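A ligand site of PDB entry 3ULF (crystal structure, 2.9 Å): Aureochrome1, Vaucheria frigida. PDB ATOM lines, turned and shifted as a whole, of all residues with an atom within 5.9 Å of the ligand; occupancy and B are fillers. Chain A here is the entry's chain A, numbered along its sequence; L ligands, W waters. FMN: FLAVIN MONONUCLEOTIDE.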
ATOM      1  N   VAL A  53     -31.223   2.332  -5.524  1.00  0.00           N
ATOM      2  CA  VAL A  53     -31.366   1.007  -4.922  1.00  0.00           C
ATOM      3  C   VAL A  53     -30.123   0.635  -4.108  1.00  0.00           C
ATOM      4  O   VAL A  53     -29.062   1.240  -4.253  1.00  0.00           O
ATOM      5  CB  VAL A  53     -31.609  -0.090  -5.977  1.00  0.00           C
ATOM      6  CG1 VAL A  53     -32.859   0.222  -6.802  1.00  0.00           C
ATOM      7  CG2 VAL A  53     -30.383  -0.250  -6.872  1.00  0.00           C
ATOM      8  N   ILE A  54     -30.285  -0.360  -3.231  1.00  0.00           N
ATOM      9  CA  ILE A  54     -29.167  -0.956  -2.501  1.00  0.00           C
ATOM     10  C   ILE A  54     -29.108  -2.436  -2.840  1.00  0.00           C
ATOM     11  O   ILE A  54     -30.108  -3.143  -2.725  1.00  0.00           O
ATOM     12  CB  ILE A  54     -29.350  -0.815  -0.964  1.00  0.00           C
ATOM     13  CG1 ILE A  54     -29.446   0.652  -0.549  1.00  0.00           C
ATOM     14  CG2 ILE A  54     -28.204  -1.488  -0.222  1.00  0.00           C
ATOM     15  CD1 ILE A  54     -28.210   1.463  -0.881  1.00  0.00           C
ATOM     16  N   THR A  55     -27.938  -2.905  -3.281  1.00  0.00           N
ATOM     17  CA  THR A  55     -27.763  -4.326  -3.553  1.00  0.00           C
ATOM     18  C   THR A  55     -26.840  -4.946  -2.524  1.00  0.00           C
ATOM     19  O   THR A  55     -26.019  -4.255  -1.926  1.00  0.00           O
ATOM     20  CB  THR A  55     -27.161  -4.564  -4.948  1.00  0.00           C
ATOM     21  OG1 THR A  55     -25.775  -4.195  -4.939  1.00  0.00           O
ATOM     22  CG2 THR A  55     -27.895  -3.741  -5.984  1.00  0.00           C
ATOM     23  N   ASP A  61     -25.279 -13.327  -6.845  1.00  0.00           N
ATOM     24  CA  ASP A  61     -25.698 -12.462  -7.946  1.00  0.00           C
ATOM     25  C   ASP A  61     -26.142 -11.070  -7.498  1.00  0.00           C
ATOM     26  O   ASP A  61     -27.033 -10.479  -8.094  1.00  0.00           O
ATOM     27  CB  ASP A  61     -26.791 -13.135  -8.777  1.00  0.00           C
ATOM     28  CG  ASP A  61     -26.874 -12.562 -10.184  1.00  0.00           C
ATOM     29  OD1 ASP A  61     -25.880 -11.957 -10.647  1.00  0.00           O
ATOM     30  OD2 ASP A  61     -27.936 -12.730 -10.824  1.00  0.00           O
ATOM     31  N   ASN A  62     -25.507 -10.545  -6.451  1.00  0.00           N
ATOM     32  CA  ASN A  62     -25.658  -9.150  -6.062  1.00  0.00           C
ATOM     33  C   ASN A  62     -27.087  -8.640  -6.264  1.00  0.00           C
ATOM     34  O   ASN A  62     -27.341  -7.791  -7.117  1.00  0.00           O
ATOM     35  CB  ASN A  62     -24.659  -8.281  -6.836  1.00  0.00           C
ATOM     36  CG  ASN A  62     -24.573  -6.871  -6.316  1.00  0.00           C
ATOM     37  OD1 ASN A  62     -24.545  -5.906  -7.094  1.00  0.00           O
ATOM     38  ND2 ASN A  62     -24.539  -6.715  -5.000  1.00  0.00           N
ATOM     39  N   PHE A  71     -37.662   4.624  -7.680  1.00  0.00           N
ATOM     40  CA  PHE A  71     -37.279   3.520  -8.546  1.00  0.00           C
ATOM     41  C   PHE A  71     -38.492   2.652  -8.874  1.00  0.00           C
ATOM     42  O   PHE A  71     -38.570   2.052  -9.939  1.00  0.00           O
ATOM     43  CB  PHE A  71     -36.186   2.682  -7.884  1.00  0.00           C
ATOM     44  CG  PHE A  71     -35.893   1.384  -8.602  1.00  0.00           C
ATOM     45  CD1 PHE A  71     -34.908   1.333  -9.581  1.00  0.00           C
ATOM     46  CD2 PHE A  71     -36.587   0.230  -8.288  1.00  0.00           C
ATOM     47  CE1 PHE A  71     -34.627   0.146 -10.236  1.00  0.00           C
ATOM     48  CE2 PHE A  71     -36.307  -0.965  -8.939  1.00  0.00           C
ATOM     49  CZ  PHE A  71     -35.327  -1.003  -9.915  1.00  0.00           C
ATOM     50  N   ASN A  86     -31.442  -9.394  -9.555  1.00  0.00           N
ATOM     51  CA  ASN A  86     -30.374  -8.577 -10.091  1.00  0.00           C
ATOM     52  C   ASN A  86     -30.955  -7.460 -10.938  1.00  0.00           C
ATOM     53  O   ASN A  86     -31.983  -7.629 -11.593  1.00  0.00           O
ATOM     54  CB  ASN A  86     -29.413  -9.419 -10.926  1.00  0.00           C
ATOM     55  CG  ASN A  86     -28.199  -8.643 -11.382  1.00  0.00           C
ATOM     56  OD1 ASN A  86     -28.266  -7.835 -12.304  1.00  0.00           O
ATOM     57  ND2 ASN A  86     -27.062  -8.879 -10.717  1.00  0.00           N
ATOM     58  N   CYS A  87     -30.302  -6.303 -10.936  1.00  0.00           N
ATOM     59  CA  CYS A  87     -30.843  -5.125 -11.622  1.00  0.00           C
ATOM     60  C   CYS A  87     -30.966  -5.310 -13.142  1.00  0.00           C
ATOM     61  O   CYS A  87     -31.635  -4.530 -13.809  1.00  0.00           O
ATOM     62  CB  CYS A  87     -30.019  -3.882 -11.275  1.00  0.00           C
ATOM     63  SG  CYS A  87     -30.664  -2.326 -11.935  1.00  0.00           S
ATOM     64  N   ARG A  88     -30.333  -6.355 -13.670  1.00  0.00           N
ATOM     65  CA  ARG A  88     -30.326  -6.583 -15.121  1.00  0.00           C
ATOM     66  C   ARG A  88     -31.721  -6.814 -15.699  1.00  0.00           C
ATOM     67  O   ARG A  88     -31.920  -6.747 -16.913  1.00  0.00           O
ATOM     68  CB  ARG A  88     -29.419  -7.778 -15.475  1.00  0.00           C
ATOM     69  CG  ARG A  88     -29.973  -9.126 -15.033  1.00  0.00           C
ATOM     70  CD  ARG A  88     -29.128 -10.285 -15.540  1.00  0.00           C
ATOM     71  NE  ARG A  88     -27.777 -10.243 -14.994  1.00  0.00           N
ATOM     72  CZ  ARG A  88     -27.395 -10.850 -13.883  1.00  0.00           C
ATOM     73  NH1 ARG A  88     -28.267 -11.568 -13.174  1.00  0.00           N
ATOM     74  NH2 ARG A  88     -26.150 -10.753 -13.465  1.00  0.00           N
ATOM     75  N   LEU A  90     -34.127  -5.039 -15.769  1.00  0.00           N
ATOM     76  CA  LEU A  90     -34.613  -3.829 -16.418  1.00  0.00           C
ATOM     77  C   LEU A  90     -34.207  -3.758 -17.887  1.00  0.00           C
ATOM     78  O   LEU A  90     -34.649  -2.873 -18.612  1.00  0.00           O
ATOM     79  CB  LEU A  90     -34.113  -2.576 -15.696  1.00  0.00           C
ATOM     80  CG  LEU A  90     -34.648  -2.333 -14.294  1.00  0.00           C
ATOM     81  CD1 LEU A  90     -34.189  -0.966 -13.812  1.00  0.00           C
ATOM     82  CD2 LEU A  90     -36.161  -2.443 -14.250  1.00  0.00           C
ATOM     83  N   GLN A  91     -33.365  -4.699 -18.318  1.00  0.00           N
ATOM     84  CA  GLN A  91     -32.850  -4.684 -19.683  1.00  0.00           C
ATOM     85  C   GLN A  91     -33.721  -5.514 -20.626  1.00  0.00           C
ATOM     86  O   GLN A  91     -34.539  -6.331 -20.193  1.00  0.00           O
ATOM     87  CB  GLN A  91     -31.407  -5.184 -19.687  1.00  0.00           C
ATOM     88  CG  GLN A  91     -30.512  -4.439 -18.702  1.00  0.00           C
ATOM     89  CD  GLN A  91     -29.136  -5.070 -18.536  1.00  0.00           C
ATOM     90  OE1 GLN A  91     -28.778  -6.012 -19.241  1.00  0.00           O
ATOM     91  NE2 GLN A  91     -28.362  -4.558 -17.585  1.00  0.00           N
ATOM     92  N   THR A  95     -31.375  -3.285 -25.581  1.00  0.00           N
ATOM     93  CA  THR A  95     -30.319  -2.817 -24.696  1.00  0.00           C
ATOM     94  C   THR A  95     -28.924  -3.083 -25.271  1.00  0.00           C
ATOM     95  O   THR A  95     -28.619  -4.215 -25.647  1.00  0.00           O
ATOM     96  CB  THR A  95     -30.436  -3.463 -23.299  1.00  0.00           C
ATOM     97  OG1 THR A  95     -31.745  -3.216 -22.758  1.00  0.00           O
ATOM     98  CG2 THR A  95     -29.398  -2.879 -22.344  1.00  0.00           C
ATOM     99  N   VAL A 100     -23.709  -2.615 -21.343  1.00  0.00           N
ATOM    100  CA  VAL A 100     -23.837  -3.578 -20.250  1.00  0.00           C
ATOM    101  C   VAL A 100     -22.471  -4.146 -19.866  1.00  0.00           C
ATOM    102  O   VAL A 100     -22.164  -4.301 -18.683  1.00  0.00           O
ATOM    103  CB  VAL A 100     -24.778  -4.746 -20.621  1.00  0.00           C
ATOM    104  CG1 VAL A 100     -24.777  -5.792 -19.519  1.00  0.00           C
ATOM    105  CG2 VAL A 100     -26.187  -4.222 -20.857  1.00  0.00           C
ATOM    106  N   ASP A 101     -21.660  -4.449 -20.866  1.00  0.00           N
ATOM    107  CA  ASP A 101     -20.319  -4.961 -20.604  1.00  0.00           C
ATOM    108  C   ASP A 101     -19.533  -3.959 -19.775  1.00  0.00           C
ATOM    109  O   ASP A 101     -18.752  -4.341 -18.902  1.00  0.00           O
ATOM    110  CB  ASP A 101     -19.591  -5.269 -21.916  1.00  0.00           C
ATOM    111  CG  ASP A 101     -20.231  -6.403 -22.693  1.00  0.00           C
ATOM    112  OD1 ASP A 101     -21.032  -7.165 -22.098  1.00  0.00           O
ATOM    113  OD2 ASP A 101     -19.928  -6.547 -23.899  1.00  0.00           O
ATOM    114  N   ILE A 103     -20.506  -1.690 -17.455  1.00  0.00           N
ATOM    115  CA  ILE A 103     -20.830  -1.764 -16.034  1.00  0.00           C
ATOM    116  C   ILE A 103     -20.334  -3.050 -15.400  1.00  0.00           C
ATOM    117  O   ILE A 103     -19.725  -3.029 -14.332  1.00  0.00           O
ATOM    118  CB  ILE A 103     -22.332  -1.657 -15.751  1.00  0.00           C
ATOM    119  CG1 ILE A 103     -23.123  -1.714 -17.064  1.00  0.00           C
ATOM    120  CG2 ILE A 103     -22.637  -0.384 -14.972  1.00  0.00           C
ATOM    121  CD1 ILE A 103     -24.598  -2.003 -16.869  1.00  0.00           C
ATOM    122  N   ARG A 104     -20.593  -4.176 -16.059  1.00  0.00           N
ATOM    123  CA  ARG A 104     -20.179  -5.452 -15.523  1.00  0.00           C
ATOM    124  C   ARG A 104     -18.691  -5.411 -15.165  1.00  0.00           C
ATOM    125  O   ARG A 104     -18.304  -5.788 -14.064  1.00  0.00           O
ATOM    126  CB  ARG A 104     -20.447  -6.592 -16.514  1.00  0.00           C
ATOM    127  CG  ARG A 104     -20.214  -7.967 -15.916  1.00  0.00           C
ATOM    128  CD  ARG A 104     -20.589  -9.078 -16.881  1.00  0.00           C
ATOM    129  NE  ARG A 104     -19.741  -9.074 -18.068  1.00  0.00           N
ATOM    130  CZ  ARG A 104     -20.101  -8.568 -19.241  1.00  0.00           C
ATOM    131  NH1 ARG A 104     -21.305  -8.023 -19.390  1.00  0.00           N
ATOM    132  NH2 ARG A 104     -19.259  -8.616 -20.261  1.00  0.00           N
ATOM    133  N   ILE A 107     -17.918  -3.053 -12.375  1.00  0.00           N
ATOM    134  CA  ILE A 107     -18.476  -3.616 -11.156  1.00  0.00           C
ATOM    135  C   ILE A 107     -17.555  -4.658 -10.528  1.00  0.00           C
ATOM    136  O   ILE A 107     -17.360  -4.671  -9.321  1.00  0.00           O
ATOM    137  CB  ILE A 107     -19.888  -4.209 -11.398  1.00  0.00           C
ATOM    138  CG1 ILE A 107     -20.945  -3.103 -11.343  1.00  0.00           C
ATOM    139  CG2 ILE A 107     -20.206  -5.279 -10.358  1.00  0.00           C
ATOM    140  CD1 ILE A 107     -22.362  -3.592 -11.513  1.00  0.00           C
ATOM    141  N   LEU A 117     -27.985   3.457 -20.641  1.00  0.00           N
ATOM    142  CA  LEU A 117     -28.477   2.388 -21.512  1.00  0.00           C
ATOM    143  C   LEU A 117     -29.996   2.349 -21.531  1.00  0.00           C
ATOM    144  O   LEU A 117     -30.663   3.026 -20.733  1.00  0.00           O
ATOM    145  CB  LEU A 117     -27.893   1.024 -21.100  1.00  0.00           C
ATOM    146  CG  LEU A 117     -27.943   0.552 -19.646  1.00  0.00           C
ATOM    147  CD1 LEU A 117     -29.372   0.315 -19.167  1.00  0.00           C
ATOM    148  CD2 LEU A 117     -27.126  -0.718 -19.518  1.00  0.00           C
ATOM    149  N   LEU A 118     -30.557   1.554 -22.440  1.00  0.00           N
ATOM    150  CA  LEU A 118     -31.994   1.474 -22.609  1.00  0.00           C
ATOM    151  C   LEU A 118     -32.569   0.423 -21.680  1.00  0.00           C
ATOM    152  O   LEU A 118     -32.145  -0.736 -21.682  1.00  0.00           O
ATOM    153  CB  LEU A 118     -32.329   1.119 -24.062  1.00  0.00           C
ATOM    154  CG  LEU A 118     -33.798   1.194 -24.476  1.00  0.00           C
ATOM    155  CD1 LEU A 118     -34.191   2.619 -24.864  1.00  0.00           C
ATOM    156  CD2 LEU A 118     -34.066   0.237 -25.622  1.00  0.00           C
ATOM    157  N   ASN A 119     -33.531   0.840 -20.864  1.00  0.00           N
ATOM    158  CA  ASN A 119     -34.222  -0.087 -19.973  1.00  0.00           C
ATOM    159  C   ASN A 119     -35.699  -0.236 -20.340  1.00  0.00           C
ATOM    160  O   ASN A 119     -36.233   0.557 -21.122  1.00  0.00           O
ATOM    161  CB  ASN A 119     -34.076   0.336 -18.510  1.00  0.00           C
ATOM    162  CG  ASN A 119     -32.725  -0.044 -17.930  1.00  0.00           C
ATOM    163  OD1 ASN A 119     -32.292   0.509 -16.915  1.00  0.00           O
ATOM    164  ND2 ASN A 119     -32.048  -0.992 -18.568  1.00  0.00           N
ATOM    165  N   ASN A 129     -31.947   5.092 -19.479  1.00  0.00           N
ATOM    166  CA  ASN A 129     -31.573   5.191 -18.078  1.00  0.00           C
ATOM    167  C   ASN A 129     -30.121   5.579 -17.917  1.00  0.00           C
ATOM    168  O   ASN A 129     -29.241   4.825 -18.323  1.00  0.00           O
ATOM    169  CB  ASN A 129     -31.824   3.851 -17.381  1.00  0.00           C
ATOM    170  CG  ASN A 129     -31.424   3.871 -15.925  1.00  0.00           C
ATOM    171  OD1 ASN A 129     -31.051   4.911 -15.380  1.00  0.00           O
ATOM    172  ND2 ASN A 129     -31.516   2.718 -15.278  1.00  0.00           N
ATOM    173  N   PHE A 131     -27.679   5.734 -15.136  1.00  0.00           N
ATOM    174  CA  PHE A 131     -27.506   5.351 -13.748  1.00  0.00           C
ATOM    175  C   PHE A 131     -26.040   5.262 -13.342  1.00  0.00           C
ATOM    176  O   PHE A 131     -25.155   5.034 -14.163  1.00  0.00           O
ATOM    177  CB  PHE A 131     -28.239   4.049 -13.429  1.00  0.00           C
ATOM    178  CG  PHE A 131     -27.593   2.821 -14.004  1.00  0.00           C
ATOM    179  CD1 PHE A 131     -26.839   1.984 -13.196  1.00  0.00           C
ATOM    180  CD2 PHE A 131     -27.730   2.503 -15.342  1.00  0.00           C
ATOM    181  CE1 PHE A 131     -26.246   0.849 -13.714  1.00  0.00           C
ATOM    182  CE2 PHE A 131     -27.137   1.368 -15.860  1.00  0.00           C
ATOM    183  CZ  PHE A 131     -26.393   0.548 -15.042  1.00  0.00           C
ATOM    184  N   PHE A 132     -25.818   5.457 -12.045  1.00  0.00           N
ATOM    185  CA  PHE A 132     -24.485   5.503 -11.473  1.00  0.00           C
ATOM    186  C   PHE A 132     -24.416   4.442 -10.380  1.00  0.00           C
ATOM    187  O   PHE A 132     -25.333   4.331  -9.572  1.00  0.00           O
ATOM    188  CB  PHE A 132     -24.228   6.893 -10.895  1.00  0.00           C
ATOM    189  CG  PHE A 132     -22.985   6.987 -10.071  1.00  0.00           C
ATOM    190  CD1 PHE A 132     -21.760   7.254 -10.669  1.00  0.00           C
ATOM    191  CD2 PHE A 132     -23.034   6.835  -8.699  1.00  0.00           C
ATOM    192  CE1 PHE A 132     -20.611   7.355  -9.907  1.00  0.00           C
ATOM    193  CE2 PHE A 132     -21.884   6.936  -7.937  1.00  0.00           C
ATOM    194  CZ  PHE A 132     -20.677   7.191  -8.541  1.00  0.00           C
ATOM    195  N   VAL A 133     -23.339   3.663 -10.382  1.00  0.00           N
ATOM    196  CA  VAL A 133     -23.183   2.635  -9.354  1.00  0.00           C
ATOM    197  C   VAL A 133     -21.863   2.819  -8.597  1.00  0.00           C
ATOM    198  O   VAL A 133     -20.829   3.109  -9.187  1.00  0.00           O
ATOM    199  CB  VAL A 133     -23.232   1.218  -9.967  1.00  0.00           C
ATOM    200  CG1 VAL A 133     -22.232   1.082 -11.092  1.00  0.00           C
ATOM    201  CG2 VAL A 133     -22.985   0.176  -8.890  1.00  0.00           C
ATOM    202  N   ALA A 134     -21.930   2.679  -7.274  1.00  0.00           N
ATOM    203  CA  ALA A 134     -20.740   2.782  -6.427  1.00  0.00           C
ATOM    204  C   ALA A 134     -20.690   1.668  -5.401  1.00  0.00           C
ATOM    205  O   ALA A 134     -21.671   1.397  -4.712  1.00  0.00           O
ATOM    206  CB  ALA A 134     -20.703   4.144  -5.747  1.00  0.00           C
ATOM    207  N   TYR A 146     -23.542  -2.423  -2.942  1.00  0.00           N
ATOM    208  CA  TYR A 146     -23.513  -1.472  -4.046  1.00  0.00           C
ATOM    209  C   TYR A 146     -24.692  -0.522  -3.933  1.00  0.00           C
ATOM    210  O   TYR A 146     -25.779  -0.898  -3.514  1.00  0.00           O
ATOM    211  CB  TYR A 146     -23.571  -2.197  -5.383  1.00  0.00           C
ATOM    212  CG  TYR A 146     -22.284  -2.864  -5.824  1.00  0.00           C
ATOM    213  CD1 TYR A 146     -21.314  -2.142  -6.517  1.00  0.00           C
ATOM    214  CD2 TYR A 146     -22.052  -4.210  -5.580  1.00  0.00           C
ATOM    215  CE1 TYR A 146     -20.139  -2.736  -6.934  1.00  0.00           C
ATOM    216  CE2 TYR A 146     -20.878  -4.812  -5.993  1.00  0.00           C
ATOM    217  CZ  TYR A 146     -19.933  -4.078  -6.670  1.00  0.00           C
ATOM    218  OH  TYR A 146     -18.759  -4.681  -7.083  1.00  0.00           O
ATOM    219  N   VAL A 147     -24.465   0.729  -4.314  1.00  0.00           N
ATOM    220  CA  VAL A 147     -25.561   1.674  -4.415  1.00  0.00           C
ATOM    221  C   VAL A 147     -25.701   2.110  -5.866  1.00  0.00           C
ATOM    222  O   VAL A 147     -24.723   2.507  -6.508  1.00  0.00           O
ATOM    223  CB  VAL A 147     -25.367   2.891  -3.498  1.00  0.00           C
ATOM    224  CG1 VAL A 147     -24.118   3.658  -3.893  1.00  0.00           C
ATOM    225  CG2 VAL A 147     -26.577   3.794  -3.562  1.00  0.00           C
ATOM    226  N   GLY A 148     -26.927   2.026  -6.389  1.00  0.00           N
ATOM    227  CA  GLY A 148     -27.206   2.475  -7.744  1.00  0.00           C
ATOM    228  C   GLY A 148     -28.148   3.663  -7.735  1.00  0.00           C
ATOM    229  O   GLY A 148     -29.076   3.736  -6.922  1.00  0.00           O
ATOM    230  N   VAL A 149     -27.914   4.603  -8.635  1.00  0.00           N
ATOM    231  CA  VAL A 149     -28.772   5.767  -8.785  1.00  0.00           C
ATOM    232  C   VAL A 149     -29.244   5.911 -10.228  1.00  0.00           C
ATOM    233  O   VAL A 149     -28.452   6.228 -11.117  1.00  0.00           O
ATOM    234  CB  VAL A 149     -28.051   7.058  -8.350  1.00  0.00           C
ATOM    235  CG1 VAL A 149     -28.919   8.257  -8.641  1.00  0.00           C
ATOM    236  CG2 VAL A 149     -27.698   6.984  -6.873  1.00  0.00           C
ATOM    237  N   GLN A 150     -30.527   5.661 -10.441  1.00  0.00           N
ATOM    238  CA  GLN A 150     -31.097   5.634 -11.784  1.00  0.00           C
ATOM    239  C   GLN A 150     -31.860   6.905 -12.123  1.00  0.00           C
ATOM    240  O   GLN A 150     -32.453   7.533 -11.239  1.00  0.00           O
ATOM    241  CB  GLN A 150     -32.027   4.432 -11.943  1.00  0.00           C
ATOM    242  CG  GLN A 150     -31.384   3.087 -11.680  1.00  0.00           C
ATOM    243  CD  GLN A 150     -31.122   2.835 -10.204  1.00  0.00           C
ATOM    244  OE1 GLN A 150     -31.740   3.459  -9.337  1.00  0.00           O
ATOM    245  NE2 GLN A 150     -30.216   1.912  -9.913  1.00  0.00           N
HETATM  246  N1  FMN L   1     -28.623  -2.456 -14.870  1.00  0.00           N
HETATM  247  C2  FMN L   1     -29.603  -1.823 -15.616  1.00  0.00           C
HETATM  248  O2  FMN L   1     -29.835  -2.220 -16.755  1.00  0.00           O
HETATM  249  N3  FMN L   1     -30.323  -0.762 -15.107  1.00  0.00           N
HETATM  250  C4  FMN L   1     -30.082  -0.300 -13.834  1.00  0.00           C
HETATM  251  O4  FMN L   1     -30.825   0.595 -13.395  1.00  0.00           O
HETATM  252  C4A FMN L   1     -29.416  -1.251 -12.827  1.00  0.00           C
HETATM  253  N5  FMN L   1     -28.733  -0.532 -11.736  1.00  0.00           N
HETATM  254  C5A FMN L   1     -27.745  -1.180 -11.017  1.00  0.00           C
HETATM  255  C6  FMN L   1     -27.459  -0.752  -9.730  1.00  0.00           C
HETATM  256  C7  FMN L   1     -26.465  -1.389  -8.986  1.00  0.00           C
HETATM  257  C7M FMN L   1     -26.272  -1.047  -7.537  1.00  0.00           C
HETATM  258  C8  FMN L   1     -25.768  -2.461  -9.548  1.00  0.00           C
HETATM  259  C8M FMN L   1     -24.707  -3.157  -8.744  1.00  0.00           C
HETATM  260  C9  FMN L   1     -26.068  -2.886 -10.834  1.00  0.00           C
HETATM  261  C9A FMN L   1     -27.061  -2.240 -11.582  1.00  0.00           C
HETATM  262  N10 FMN L   1     -27.347  -2.668 -12.869  1.00  0.00           N
HETATM  263  C10 FMN L   1     -28.339  -2.034 -13.596  1.00  0.00           C
HETATM  264  C1' FMN L   1     -26.324  -3.470 -13.625  1.00  0.00           C
HETATM  265  C2' FMN L   1     -26.723  -4.943 -13.731  1.00  0.00           C
HETATM  266  O2' FMN L   1     -27.343  -5.376 -12.541  1.00  0.00           O
HETATM  267  C3' FMN L   1     -25.506  -5.800 -14.053  1.00  0.00           C
HETATM  268  O3' FMN L   1     -24.522  -5.577 -13.073  1.00  0.00           O
HETATM  269  C4' FMN L   1     -24.972  -5.450 -15.440  1.00  0.00           C
HETATM  270  O4' FMN L   1     -26.012  -5.615 -16.387  1.00  0.00           O
HETATM  271  C5' FMN L   1     -23.821  -6.338 -15.892  1.00  0.00           C
HETATM  272  O5' FMN L   1     -23.963  -7.595 -15.289  1.00  0.00           O
HETATM  273  P   FMN L   1     -24.358  -8.882 -16.162  1.00  0.00           P
HETATM  274  O1P FMN L   1     -25.852  -8.848 -16.346  1.00  0.00           O
HETATM  275  O2P FMN L   1     -23.961 -10.143 -15.438  1.00  0.00           O
HETATM  276  O3P FMN L   1     -23.673  -8.805 -17.505  1.00  0.00           O
HETATM  277  O   HOH W   1     -27.660  -6.411  -9.338  1.00  0.00           O
HETATM  278  O   HOH W   2     -24.446  -6.679 -10.591  1.00  0.00           O
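The guanidinium group (NE) of Arg 88 lies within salt-bridge range of an oxygen (O1P) of the ligand.
The backbone NH (N) of Cys 87 sits close to an oxygen (O2') of the ligand (3.5 Å).
The guanidinium group of Arg 104 is in salt-bridge range of an oxygen (O3P) of the ligand.
NE2 of Gln 150 is in hydrogen-bond range of N5 of the ligand (3.4 Å).
The side-chain amide nitrogen (ND2) of Asn 129 lies within hydrogen-bond range of an oxygen (O4) of the ligand, at 2.9 Å.
N of Arg 88 is in hydrogen-bond range of O2' of the ligand, 3.3 Å away.
SG of Cys 87 is bonded to C4A of the ligand (1.9 Å).
The side-chain amide oxygen of Asn 86 sits at hydrogen-bond distance from an oxygen (O2') of the ligand (2.6 Å).
OD1 of Asn 119 sits at hydrogen-bond distance from N3 of the ligand, 3.0 Å away.
NE2 of Gln 91 is in hydrogen-bond range of O4' of the ligand.
The side-chain amide nitrogen of Asn 86 sits at hydrogen-bond distance from the backbone carbonyl oxygen of Asp 61 (3.1 Å).
ND2 of Asn 129 is in hydrogen-bond range of OD1 of Asn 119 (2.9 Å).
The backbone NH of Val 147 is in hydrogen-bond range of the backbone carbonyl oxygen of Ala 134 (2.9 Å).
OD1 of Asn 86 is in hydrogen-bond range of N of Arg 88 (2.9 Å).
O of Gly 148 sits at hydrogen-bond distance from N of Val 53 (2.9 Å).
The backbone NH of Asn 129 is in hydrogen-bond range of the backbone carbonyl oxygen of Leu 117 (2.7 Å).
OD1 of Asn 129 sits at hydrogen-bond distance from N of Phe 131 (3.5 Å).
The backbone carbonyl oxygen (O) of Tyr 146 is in hydrogen-bond range of the backbone NH (N) of Thr 55, at 3.0 Å.
Thr 55 touches the ligand (CG2 to C7M, 3.5 Å).
Asn 62 touches the ligand (OD1 to C8M, 3.2 Å).
Leu 90 touches the ligand.
Val 100 touches the ligand.
Ile 103 touches the ligand (CD1 to C4', 3.8 Å).
Ile 107 touches the ligand (CD1 to O3', 3.3 Å).
Leu 117 touches the ligand (CD1 to O2, 3.5 Å).
Phe 131 touches the ligand (CE1 to N5, 3.5 Å).
Val 133 touches the ligand.
CB of Tyr 146 touches C7M of the ligand, 3.6 Å away.
C of Val 147 touches C7M of the ligand, at 3.6 Å.
N of Gly 148 touches C7M of the ligand (3.3 Å).
Hydrophobic or aromatic side chains within 4 Å of the ligand: Leu 90, Val 100, Ile 103, Ile 107, Leu 117, Phe 131, Val 133 and Tyr 146.
Within 4 Å of the ligand: Thr 55, Asn 62, Asn 86, Cys 87, Arg 88, Leu 90, Gln 91, Val 100, Ile 103, Arg 104, Ile 107, Leu 117, Asn 119, Asn 129, Phe 131, Val 133, Tyr 146, Val 147, Gly 148 and Gln 150.
Water W2 lies within hydrogen-bond range of O3' of the ligand and ND2 of Asn 86.
Water W1 lies within hydrogen-bond range of O of Asn 62 (2.6 Å), ND2 of Asn 86 (2.9 Å), N of Cys 87 (3.1 Å) and O2' of the ligand (3.4 Å).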
